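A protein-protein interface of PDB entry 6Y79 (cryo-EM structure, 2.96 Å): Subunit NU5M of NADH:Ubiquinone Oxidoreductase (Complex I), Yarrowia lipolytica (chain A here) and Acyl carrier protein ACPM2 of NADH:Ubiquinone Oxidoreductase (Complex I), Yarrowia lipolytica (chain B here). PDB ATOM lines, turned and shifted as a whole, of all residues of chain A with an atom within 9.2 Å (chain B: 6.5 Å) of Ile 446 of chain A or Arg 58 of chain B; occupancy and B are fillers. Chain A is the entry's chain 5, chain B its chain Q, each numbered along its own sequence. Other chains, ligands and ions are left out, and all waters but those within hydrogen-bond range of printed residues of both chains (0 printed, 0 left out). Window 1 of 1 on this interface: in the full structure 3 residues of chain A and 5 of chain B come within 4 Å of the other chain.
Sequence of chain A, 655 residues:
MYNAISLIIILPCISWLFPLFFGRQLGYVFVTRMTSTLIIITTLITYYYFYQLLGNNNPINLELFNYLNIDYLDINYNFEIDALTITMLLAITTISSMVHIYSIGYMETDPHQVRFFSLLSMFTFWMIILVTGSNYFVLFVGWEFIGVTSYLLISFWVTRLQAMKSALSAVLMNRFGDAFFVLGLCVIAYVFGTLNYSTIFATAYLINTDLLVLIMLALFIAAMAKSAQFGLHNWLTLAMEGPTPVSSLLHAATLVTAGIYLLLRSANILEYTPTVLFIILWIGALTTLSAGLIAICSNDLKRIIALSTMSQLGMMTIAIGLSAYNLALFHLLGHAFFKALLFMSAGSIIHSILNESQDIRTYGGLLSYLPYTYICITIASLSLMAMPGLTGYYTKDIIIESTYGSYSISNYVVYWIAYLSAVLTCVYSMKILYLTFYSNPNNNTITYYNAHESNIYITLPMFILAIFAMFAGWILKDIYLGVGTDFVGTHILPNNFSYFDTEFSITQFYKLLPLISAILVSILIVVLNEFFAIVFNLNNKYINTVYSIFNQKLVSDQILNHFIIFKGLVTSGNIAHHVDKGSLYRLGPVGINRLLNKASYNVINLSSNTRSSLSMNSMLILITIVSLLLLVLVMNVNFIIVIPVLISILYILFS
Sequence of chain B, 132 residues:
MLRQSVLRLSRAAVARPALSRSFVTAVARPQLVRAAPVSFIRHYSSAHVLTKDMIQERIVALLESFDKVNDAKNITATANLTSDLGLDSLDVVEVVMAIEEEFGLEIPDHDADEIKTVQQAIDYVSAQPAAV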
ATOM      1  N   SER A 352      22.183  13.083  35.868  1.00  0.00           N
ATOM      2  CA  SER A 352      20.801  13.420  36.173  1.00  0.00           C
ATOM      3  C   SER A 352      19.847  12.982  35.069  1.00  0.00           C
ATOM      4  O   SER A 352      18.697  12.638  35.351  1.00  0.00           O
ATOM      5  CB  SER A 352      20.682  14.921  36.420  1.00  0.00           C
ATOM      6  OG  SER A 352      19.335  15.314  36.561  1.00  0.00           O
ATOM      7  N   ILE A 353      20.301  12.984  33.821  1.00  0.00           N
ATOM      8  CA  ILE A 353      19.480  12.522  32.709  1.00  0.00           C
ATOM      9  C   ILE A 353      19.344  11.006  32.776  1.00  0.00           C
ATOM     10  O   ILE A 353      20.336  10.289  32.959  1.00  0.00           O
ATOM     11  CB  ILE A 353      20.095  12.999  31.382  1.00  0.00           C
ATOM     12  CG1 ILE A 353      19.974  14.515  31.283  1.00  0.00           C
ATOM     13  CG2 ILE A 353      19.442  12.359  30.193  1.00  0.00           C
ATOM     14  CD1 ILE A 353      20.621  15.090  30.054  1.00  0.00           C
ATOM     15  N   LEU A 354      18.101  10.516  32.658  1.00  0.00           N
ATOM     16  CA  LEU A 354      17.824   9.078  32.632  1.00  0.00           C
ATOM     17  C   LEU A 354      18.509   8.393  31.460  1.00  0.00           C
ATOM     18  O   LEU A 354      18.919   7.234  31.570  1.00  0.00           O
ATOM     19  CB  LEU A 354      16.310   8.842  32.554  1.00  0.00           C
ATOM     20  CG  LEU A 354      15.668   7.455  32.731  1.00  0.00           C
ATOM     21  CD1 LEU A 354      14.300   7.631  33.349  1.00  0.00           C
ATOM     22  CD2 LEU A 354      15.530   6.644  31.442  1.00  0.00           C
ATOM     23  N   ASN A 355      18.630   9.095  30.336  1.00  0.00           N
ATOM     24  CA  ASN A 355      19.236   8.525  29.138  1.00  0.00           C
ATOM     25  C   ASN A 355      20.728   8.286  29.323  1.00  0.00           C
ATOM     26  O   ASN A 355      21.275   7.337  28.753  1.00  0.00           O
ATOM     27  CB  ASN A 355      18.988   9.458  27.955  1.00  0.00           C
ATOM     28  CG  ASN A 355      19.378   8.847  26.636  1.00  0.00           C
ATOM     29  OD1 ASN A 355      19.513   7.632  26.513  1.00  0.00           O
ATOM     30  ND2 ASN A 355      19.565   9.693  25.633  1.00  0.00           N
ATOM     31  N   TYR A 369      14.876  22.745  36.133  1.00  0.00           N
ATOM     32  CA  TYR A 369      14.952  21.446  36.785  1.00  0.00           C
ATOM     33  C   TYR A 369      16.226  21.268  37.591  1.00  0.00           C
ATOM     34  O   TYR A 369      16.230  20.523  38.577  1.00  0.00           O
ATOM     35  CB  TYR A 369      14.851  20.336  35.736  1.00  0.00           C
ATOM     36  CG  TYR A 369      13.520  20.261  35.015  1.00  0.00           C
ATOM     37  CD1 TYR A 369      12.390  20.855  35.531  1.00  0.00           C
ATOM     38  CD2 TYR A 369      13.402  19.616  33.804  1.00  0.00           C
ATOM     39  CE1 TYR A 369      11.176  20.795  34.886  1.00  0.00           C
ATOM     40  CE2 TYR A 369      12.187  19.559  33.154  1.00  0.00           C
ATOM     41  CZ  TYR A 369      11.081  20.145  33.695  1.00  0.00           C
ATOM     42  OH  TYR A 369       9.875  20.083  33.036  1.00  0.00           O
ATOM     43  N   ASN A 443      15.129  16.539  24.405  1.00  0.00           N
ATOM     44  CA  ASN A 443      14.964  15.158  24.815  1.00  0.00           C
ATOM     45  C   ASN A 443      13.483  14.805  24.897  1.00  0.00           C
ATOM     46  O   ASN A 443      12.608  15.667  24.799  1.00  0.00           O
ATOM     47  CB  ASN A 443      15.650  14.923  26.156  1.00  0.00           C
ATOM     48  CG  ASN A 443      16.261  13.546  26.262  1.00  0.00           C
ATOM     49  OD1 ASN A 443      15.986  12.667  25.450  1.00  0.00           O
ATOM     50  ND2 ASN A 443      17.114  13.358  27.253  1.00  0.00           N
ATOM     51  N   ASN A 444      13.201  13.517  25.073  1.00  0.00           N
ATOM     52  CA  ASN A 444      11.819  13.097  25.248  1.00  0.00           C
ATOM     53  C   ASN A 444      11.325  13.480  26.643  1.00  0.00           C
ATOM     54  O   ASN A 444      12.104  13.826  27.532  1.00  0.00           O
ATOM     55  CB  ASN A 444      11.669  11.596  24.992  1.00  0.00           C
ATOM     56  CG  ASN A 444      12.573  10.743  25.862  1.00  0.00           C
ATOM     57  OD1 ASN A 444      13.369  11.241  26.654  1.00  0.00           O
ATOM     58  ND2 ASN A 444      12.444   9.432  25.717  1.00  0.00           N
ATOM     59  N   THR A 445      10.006  13.393  26.830  1.00  0.00           N
ATOM     60  CA  THR A 445       9.364  14.017  27.983  1.00  0.00           C
ATOM     61  C   THR A 445       9.681  13.319  29.300  1.00  0.00           C
ATOM     62  O   THR A 445       9.657  13.962  30.356  1.00  0.00           O
ATOM     63  CB  THR A 445       7.847  14.080  27.755  1.00  0.00           C
ATOM     64  OG1 THR A 445       7.224  14.768  28.841  1.00  0.00           O
ATOM     65  CG2 THR A 445       7.235  12.688  27.615  1.00  0.00           C
ATOM     66  N   ILE A 446      10.051  12.041  29.252  1.00  0.00           N
ATOM     67  CA  ILE A 446      10.189  11.259  30.469  1.00  0.00           C
ATOM     68  C   ILE A 446      11.491  11.584  31.201  1.00  0.00           C
ATOM     69  O   ILE A 446      11.551  11.504  32.437  1.00  0.00           O
ATOM     70  CB  ILE A 446      10.064   9.772  30.112  1.00  0.00           C
ATOM     71  CG1 ILE A 446      10.074   8.924  31.371  1.00  0.00           C
ATOM     72  CG2 ILE A 446      11.124   9.341  29.099  1.00  0.00           C
ATOM     73  CD1 ILE A 446       9.927   7.532  31.082  1.00  0.00           C
ATOM     74  N   THR A 447      12.534  11.977  30.463  1.00  0.00           N
ATOM     75  CA  THR A 447      13.730  12.560  31.050  1.00  0.00           C
ATOM     76  C   THR A 447      13.403  13.798  31.863  1.00  0.00           C
ATOM     77  O   THR A 447      13.910  13.960  32.977  1.00  0.00           O
ATOM     78  CB  THR A 447      14.712  12.910  29.935  1.00  0.00           C
ATOM     79  OG1 THR A 447      15.072  11.719  29.226  1.00  0.00           O
ATOM     80  CG2 THR A 447      15.953  13.551  30.492  1.00  0.00           C
ATOM     81  N   TYR A 448      12.505  14.631  31.356  1.00  0.00           N
ATOM     82  CA  TYR A 448      12.096  15.819  32.077  1.00  0.00           C
ATOM     83  C   TYR A 448      11.167  15.491  33.239  1.00  0.00           C
ATOM     84  O   TYR A 448      11.064  16.283  34.182  1.00  0.00           O
ATOM     85  CB  TYR A 448      11.464  16.792  31.088  1.00  0.00           C
ATOM     86  CG  TYR A 448      12.462  17.252  30.052  1.00  0.00           C
ATOM     87  CD1 TYR A 448      13.474  18.135  30.389  1.00  0.00           C
ATOM     88  CD2 TYR A 448      12.415  16.784  28.750  1.00  0.00           C
ATOM     89  CE1 TYR A 448      14.393  18.560  29.468  1.00  0.00           C
ATOM     90  CE2 TYR A 448      13.339  17.204  27.814  1.00  0.00           C
ATOM     91  CZ  TYR A 448      14.328  18.090  28.188  1.00  0.00           C
ATOM     92  OH  TYR A 448      15.257  18.523  27.278  1.00  0.00           O
ATOM     93  N   TYR A 449      10.490  14.339  33.204  1.00  0.00           N
ATOM     94  CA  TYR A 449       9.787  13.888  34.406  1.00  0.00           C
ATOM     95  C   TYR A 449      10.761  13.438  35.485  1.00  0.00           C
ATOM     96  O   TYR A 449      10.569  13.743  36.667  1.00  0.00           O
ATOM     97  CB  TYR A 449       8.822  12.747  34.087  1.00  0.00           C
ATOM     98  CG  TYR A 449       7.564  13.181  33.388  1.00  0.00           C
ATOM     99  CD1 TYR A 449       6.614  13.960  34.036  1.00  0.00           C
ATOM    100  CD2 TYR A 449       7.320  12.797  32.083  1.00  0.00           C
ATOM    101  CE1 TYR A 449       5.464  14.351  33.388  1.00  0.00           C
ATOM    102  CE2 TYR A 449       6.186  13.185  31.429  1.00  0.00           C
ATOM    103  CZ  TYR A 449       5.264  13.963  32.083  1.00  0.00           C
ATOM    104  OH  TYR A 449       4.131  14.344  31.420  1.00  0.00           O
ATOM    105  N   ASN A 450      11.807  12.711  35.102  1.00  0.00           N
ATOM    106  CA  ASN A 450      12.689  12.054  36.055  1.00  0.00           C
ATOM    107  C   ASN A 450      13.953  12.848  36.355  1.00  0.00           C
ATOM    108  O   ASN A 450      14.842  12.330  37.037  1.00  0.00           O
ATOM    109  CB  ASN A 450      13.068  10.665  35.547  1.00  0.00           C
ATOM    110  CG  ASN A 450      11.878   9.741  35.449  1.00  0.00           C
ATOM    111  OD1 ASN A 450      11.540   9.260  34.370  1.00  0.00           O
ATOM    112  ND2 ASN A 450      11.233   9.489  36.578  1.00  0.00           N
ATOM    113  N   ALA A 451      14.061  14.079  35.866  1.00  0.00           N
ATOM    114  CA  ALA A 451      15.215  14.907  36.189  1.00  0.00           C
ATOM    115  C   ALA A 451      15.102  15.400  37.623  1.00  0.00           C
ATOM    116  O   ALA A 451      14.166  16.125  37.972  1.00  0.00           O
ATOM    117  CB  ALA A 451      15.326  16.082  35.224  1.00  0.00           C
ATOM    118  N   HIS A 452      16.055  14.991  38.449  1.00  0.00           N
ATOM    119  CA  HIS A 452      16.134  15.392  39.841  1.00  0.00           C
ATOM    120  C   HIS A 452      17.585  15.725  40.129  1.00  0.00           C
ATOM    121  O   HIS A 452      18.462  15.539  39.282  1.00  0.00           O
ATOM    122  CB  HIS A 452      15.621  14.288  40.774  1.00  0.00           C
ATOM    123  CG  HIS A 452      16.404  13.018  40.681  1.00  0.00           C
ATOM    124  ND1 HIS A 452      16.306  12.160  39.608  1.00  0.00           N
ATOM    125  CD2 HIS A 452      17.313  12.468  41.518  1.00  0.00           C
ATOM    126  CE1 HIS A 452      17.118  11.136  39.788  1.00  0.00           C
ATOM    127  NE2 HIS A 452      17.741  11.298  40.939  1.00  0.00           N
ATOM    128  N   HIS B  48      14.187   3.748  37.353  1.00  0.00           N
ATOM    129  CA  HIS B  48      12.922   3.891  36.650  1.00  0.00           C
ATOM    130  C   HIS B  48      12.682   2.648  35.813  1.00  0.00           C
ATOM    131  O   HIS B  48      13.462   2.332  34.905  1.00  0.00           O
ATOM    132  CB  HIS B  48      12.882   5.136  35.779  1.00  0.00           C
ATOM    133  CG  HIS B  48      11.585   5.285  35.057  1.00  0.00           C
ATOM    134  ND1 HIS B  48      10.404   5.560  35.713  1.00  0.00           N
ATOM    135  CD2 HIS B  48      11.276   5.192  33.745  1.00  0.00           C
ATOM    136  CE1 HIS B  48       9.424   5.634  34.832  1.00  0.00           C
ATOM    137  NE2 HIS B  48       9.926   5.411  33.633  1.00  0.00           N
ATOM    138  N   LEU B  50      10.273   0.486  33.206  1.00  0.00           N
ATOM    139  CA  LEU B  50       9.085   0.439  32.401  1.00  0.00           C
ATOM    140  C   LEU B  50       8.433  -0.920  32.546  1.00  0.00           C
ATOM    141  O   LEU B  50       9.034  -1.906  32.986  1.00  0.00           O
ATOM    142  CB  LEU B  50       9.382   0.782  30.942  1.00  0.00           C
ATOM    143  CG  LEU B  50      10.271   0.031  29.928  1.00  0.00           C
ATOM    144  CD1 LEU B  50       9.601  -1.201  29.354  1.00  0.00           C
ATOM    145  CD2 LEU B  50      10.569   0.971  28.784  1.00  0.00           C
ATOM    146  N   ASP B  53       2.332  -1.793  30.072  1.00  0.00           N
ATOM    147  CA  ASP B  53       1.282  -0.791  30.215  1.00  0.00           C
ATOM    148  C   ASP B  53       1.757   0.571  29.734  1.00  0.00           C
ATOM    149  O   ASP B  53       1.023   1.308  29.061  1.00  0.00           O
ATOM    150  CB  ASP B  53       0.814  -0.726  31.674  1.00  0.00           C
ATOM    151  CG  ASP B  53       1.945  -0.395  32.673  1.00  0.00           C
ATOM    152  OD1 ASP B  53       3.124  -0.239  32.276  1.00  0.00           O
ATOM    153  OD2 ASP B  53       1.671  -0.242  33.901  1.00  0.00           O
ATOM    154  N   MET B  54       3.003   0.875  30.052  1.00  0.00           N
ATOM    155  CA  MET B  54       3.573   2.177  29.799  1.00  0.00           C
ATOM    156  C   MET B  54       3.885   2.366  28.326  1.00  0.00           C
ATOM    157  O   MET B  54       3.548   3.398  27.751  1.00  0.00           O
ATOM    158  CB  MET B  54       4.816   2.307  30.652  1.00  0.00           C
ATOM    159  CG  MET B  54       5.330   3.644  30.673  1.00  0.00           C
ATOM    160  SD  MET B  54       6.389   3.712  32.089  1.00  0.00           S
ATOM    161  CE  MET B  54       7.449   4.970  31.397  1.00  0.00           C
ATOM    162  N   ILE B  55       4.549   1.381  27.710  1.00  0.00           N
ATOM    163  CA  ILE B  55       4.784   1.373  26.265  1.00  0.00           C
ATOM    164  C   ILE B  55       3.474   1.489  25.510  1.00  0.00           C
ATOM    165  O   ILE B  55       3.380   2.222  24.517  1.00  0.00           O
ATOM    166  CB  ILE B  55       5.523   0.088  25.858  1.00  0.00           C
ATOM    167  CG1 ILE B  55       6.804  -0.088  26.676  1.00  0.00           C
ATOM    168  CG2 ILE B  55       5.861   0.098  24.392  1.00  0.00           C
ATOM    169  CD1 ILE B  55       7.616  -1.272  26.254  1.00  0.00           C
ATOM    170  N   GLN B  56       2.435   0.803  26.003  1.00  0.00           N
ATOM    171  CA  GLN B  56       1.095   0.916  25.431  1.00  0.00           C
ATOM    172  C   GLN B  56       0.590   2.357  25.464  1.00  0.00           C
ATOM    173  O   GLN B  56       0.294   2.955  24.417  1.00  0.00           O
ATOM    174  CB  GLN B  56       0.135  -0.004  26.187  1.00  0.00           C
ATOM    175  CG  GLN B  56      -1.278   0.028  25.660  1.00  0.00           C
ATOM    176  CD  GLN B  56      -1.422  -0.730  24.354  1.00  0.00           C
ATOM    177  OE1 GLN B  56      -0.831  -1.797  24.179  1.00  0.00           O
ATOM    178  NE2 GLN B  56      -2.216  -0.185  23.433  1.00  0.00           N
ATOM    179  N   GLU B  57       0.529   2.949  26.658  1.00  0.00           N
ATOM    180  CA  GLU B  57      -0.034   4.287  26.746  1.00  0.00           C
ATOM    181  C   GLU B  57       0.913   5.378  26.269  1.00  0.00           C
ATOM    182  O   GLU B  57       0.503   6.541  26.253  1.00  0.00           O
ATOM    183  CB  GLU B  57      -0.499   4.598  28.163  1.00  0.00           C
ATOM    184  CG  GLU B  57       0.585   4.661  29.199  1.00  0.00           C
ATOM    185  CD  GLU B  57       0.002   4.786  30.586  1.00  0.00           C
ATOM    186  OE1 GLU B  57      -1.186   5.154  30.694  1.00  0.00           O
ATOM    187  OE2 GLU B  57       0.724   4.507  31.564  1.00  0.00           O
ATOM    188  N   ARG B  58       2.156   5.052  25.901  1.00  0.00           N
ATOM    189  CA  ARG B  58       3.016   6.024  25.231  1.00  0.00           C
ATOM    190  C   ARG B  58       2.903   5.961  23.719  1.00  0.00           C
ATOM    191  O   ARG B  58       2.839   7.014  23.071  1.00  0.00           O
ATOM    192  CB  ARG B  58       4.478   5.833  25.646  1.00  0.00           C
ATOM    193  CG  ARG B  58       4.749   6.229  27.079  1.00  0.00           C
ATOM    194  CD  ARG B  58       6.214   6.179  27.414  1.00  0.00           C
ATOM    195  NE  ARG B  58       6.872   7.419  27.036  1.00  0.00           N
ATOM    196  CZ  ARG B  58       8.160   7.665  27.224  1.00  0.00           C
ATOM    197  NH1 ARG B  58       8.938   6.752  27.791  1.00  0.00           N
ATOM    198  NH2 ARG B  58       8.662   8.829  26.847  1.00  0.00           N
ATOM    199  N   ILE B  59       2.864   4.753  23.139  1.00  0.00           N
ATOM    200  CA  ILE B  59       2.732   4.621  21.682  1.00  0.00           C
ATOM    201  C   ILE B  59       1.345   5.074  21.210  1.00  0.00           C
ATOM    202  O   ILE B  59       1.218   5.765  20.180  1.00  0.00           O
ATOM    203  CB  ILE B  59       3.028   3.170  21.257  1.00  0.00           C
ATOM    204  CG1 ILE B  59       4.501   2.850  21.527  1.00  0.00           C
ATOM    205  CG2 ILE B  59       2.773   2.924  19.810  1.00  0.00           C
ATOM    206  CD1 ILE B  59       4.892   1.440  21.191  1.00  0.00           C
ATOM    207  N   VAL B  60       0.275   4.774  21.981  1.00  0.00           N
ATOM    208  CA  VAL B  60      -1.024   5.336  21.643  1.00  0.00           C
ATOM    209  C   VAL B  60      -1.073   6.845  21.857  1.00  0.00           C
ATOM    210  O   VAL B  60      -1.730   7.526  21.083  1.00  0.00           O
ATOM    211  CB  VAL B  60      -2.171   4.611  22.374  1.00  0.00           C
ATOM    212  CG1 VAL B  60      -2.106   3.111  22.188  1.00  0.00           C
ATOM    213  CG2 VAL B  60      -2.239   4.994  23.846  1.00  0.00           C
ATOM    214  N   ALA B  61      -0.316   7.387  22.811  1.00  0.00           N
ATOM    215  CA  ALA B  61      -0.286   8.821  23.028  1.00  0.00           C
ATOM    216  C   ALA B  61       0.379   9.514  21.854  1.00  0.00           C
ATOM    217  O   ALA B  61      -0.159  10.508  21.312  1.00  0.00           O
ATOM    218  CB  ALA B  61       0.460   9.159  24.350  1.00  0.00           C
ATOM    219  N   LEU B  62       1.475   8.904  21.392  1.00  0.00           N
ATOM    220  CA  LEU B  62       2.184   9.330  20.207  1.00  0.00           C
ATOM    221  C   LEU B  62       1.275   9.314  18.990  1.00  0.00           C
ATOM    222  O   LEU B  62       1.308  10.240  18.177  1.00  0.00           O
ATOM    223  CB  LEU B  62       3.378   8.406  20.029  1.00  0.00           C
ATOM    224  CG  LEU B  62       4.358   8.724  18.909  1.00  0.00           C
ATOM    225  CD1 LEU B  62       5.029  10.022  19.273  1.00  0.00           C
ATOM    226  CD2 LEU B  62       5.325   7.585  18.902  1.00  0.00           C
ATOM    227  N   LEU B  63       0.444   8.278  18.849  1.00  0.00           N
ATOM    228  CA  LEU B  63      -0.418   8.213  17.670  1.00  0.00           C
ATOM    229  C   LEU B  63      -1.634   9.127  17.739  1.00  0.00           C
ATOM    230  O   LEU B  63      -2.134   9.520  16.681  1.00  0.00           O
ATOM    231  CB  LEU B  63      -0.859   6.777  17.419  1.00  0.00           C
ATOM    232  CG  LEU B  63       0.255   5.912  16.826  1.00  0.00           C
ATOM    233  CD1 LEU B  63      -0.122   4.445  16.861  1.00  0.00           C
ATOM    234  CD2 LEU B  63       0.586   6.354  15.408  1.00  0.00           C
ATOM    235  N   GLU B 102      11.063   8.763  20.530  1.00  0.00           N
ATOM    236  CA  GLU B 102      10.200   8.756  21.704  1.00  0.00           C
ATOM    237  C   GLU B 102      10.770   7.865  22.804  1.00  0.00           C
ATOM    238  O   GLU B 102      10.851   8.274  23.965  1.00  0.00           O
ATOM    239  CB  GLU B 102       8.814   8.279  21.303  1.00  0.00           C
ATOM    240  CG  GLU B 102       7.798   8.145  22.429  1.00  0.00           C
ATOM    241  CD  GLU B 102       7.681   9.391  23.276  1.00  0.00           C
ATOM    242  OE1 GLU B 102       7.059  10.359  22.797  1.00  0.00           O
ATOM    243  OE2 GLU B 102       8.164   9.389  24.428  1.00  0.00           O
ATOM    244  N   PHE B 103      11.204   6.661  22.459  1.00  0.00           N
ATOM    245  CA  PHE B 103      11.745   5.738  23.449  1.00  0.00           C
ATOM    246  C   PHE B 103      13.231   5.918  23.685  1.00  0.00           C
ATOM    247  O   PHE B 103      13.797   5.207  24.519  1.00  0.00           O
ATOM    248  CB  PHE B 103      11.450   4.298  23.032  1.00  0.00           C
ATOM    249  CG  PHE B 103      10.023   3.937  23.190  1.00  0.00           C
ATOM    250  CD1 PHE B 103       9.470   3.815  24.453  1.00  0.00           C
ATOM    251  CD2 PHE B 103       9.221   3.757  22.086  1.00  0.00           C
ATOM    252  CE1 PHE B 103       8.156   3.499  24.609  1.00  0.00           C
ATOM    253  CE2 PHE B 103       7.909   3.433  22.242  1.00  0.00           C
ATOM    254  CZ  PHE B 103       7.377   3.308  23.509  1.00  0.00           C
ATOM    255  N   ALA B 131      15.700   2.243  27.740  1.00  0.00           N
ATOM    256  CA  ALA B 131      14.389   2.857  27.886  1.00  0.00           C
ATOM    257  C   ALA B 131      14.447   4.350  27.617  1.00  0.00           C
ATOM    258  O   ALA B 131      13.937   5.145  28.408  1.00  0.00           O
ATOM    259  CB  ALA B 131      13.844   2.600  29.281  1.00  0.00           C
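The side-chain amide nitrogen (ND2) of Asn 444 of chain A sits at hydrogen-bond distance from the backbone carbonyl oxygen (O) of Glu 102 of chain B (2.6 Å).
The side-chain amide oxygen of Asn 443 of chain A lies close to the side-chain amide oxygen of Asn 444 of chain A (3.2 Å). The side-chain amide oxygen (OD1) of Asn 444 of chain A is in hydrogen-bond range of the side-chain hydroxyl (OG1) of Thr 447 of chain A, at 3.1 Å. The side-chain carboxylate (OE2) of Glu 102 of chain B is in salt-bridge range of the guanidinium group (NH2) of Arg 58 of chain B, at 2.5 Å. OD1 of Asn 450 of chain A lies close to O of Ile 446 of chain A (3.0 Å).
Leu 354 of chain A touches His 48 of chain B. Ala 131 of chain B touches Leu 354 of chain A (O to CD2, 3.7 Å). ND2 of Asn 444 of chain A touches NH2 of Arg 58 of chain B (3.99 Å). Ile 446 of chain A touches His 48 of chain B. Met 54 of chain B touches Ile 446 of chain A. Ile 446 of chain A touches Arg 58 of chain B.
Ile 446 of chain A touches just these residues of chain B: His 48 (3.3 Å), Met 54 (3.6 Å) and Arg 58 (3.4 Å). Printed residues of chain A within 4 Å of Arg 58 of chain B: Asn 444 and Ile 446. Of the printed residues of chain A, His 48 of chain B touches Leu 354 (3.8 Å) and Ile 446 (3.3 Å). Of the printed residues of chain A, Ala 131 of chain B touches Leu 354. Printed residues of chain A within 4 Å of Glu 102 of chain B: Asn 444. Ile 353 of chain A touches none of the printed residues of chain B. The nearest residue of chain B that does not touch Ile 446 of chain A is Ala 131 of chain B (5.1 Å).
Hydrophobic or aromatic side chains of chain B within 4 Å of the printed part of chain A: His 48 and Met 54. Hydrophobic or aromatic side chains of chain A within 4 Å of the printed part of chain B: Leu 354 and Ile 446. Among the printed residues, 7 pairs touch across the chains. Among the printed residues, no Asp or Glu carboxylate lies within 4 Å of a Lys or Arg side-chain nitrogen of the other chain.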
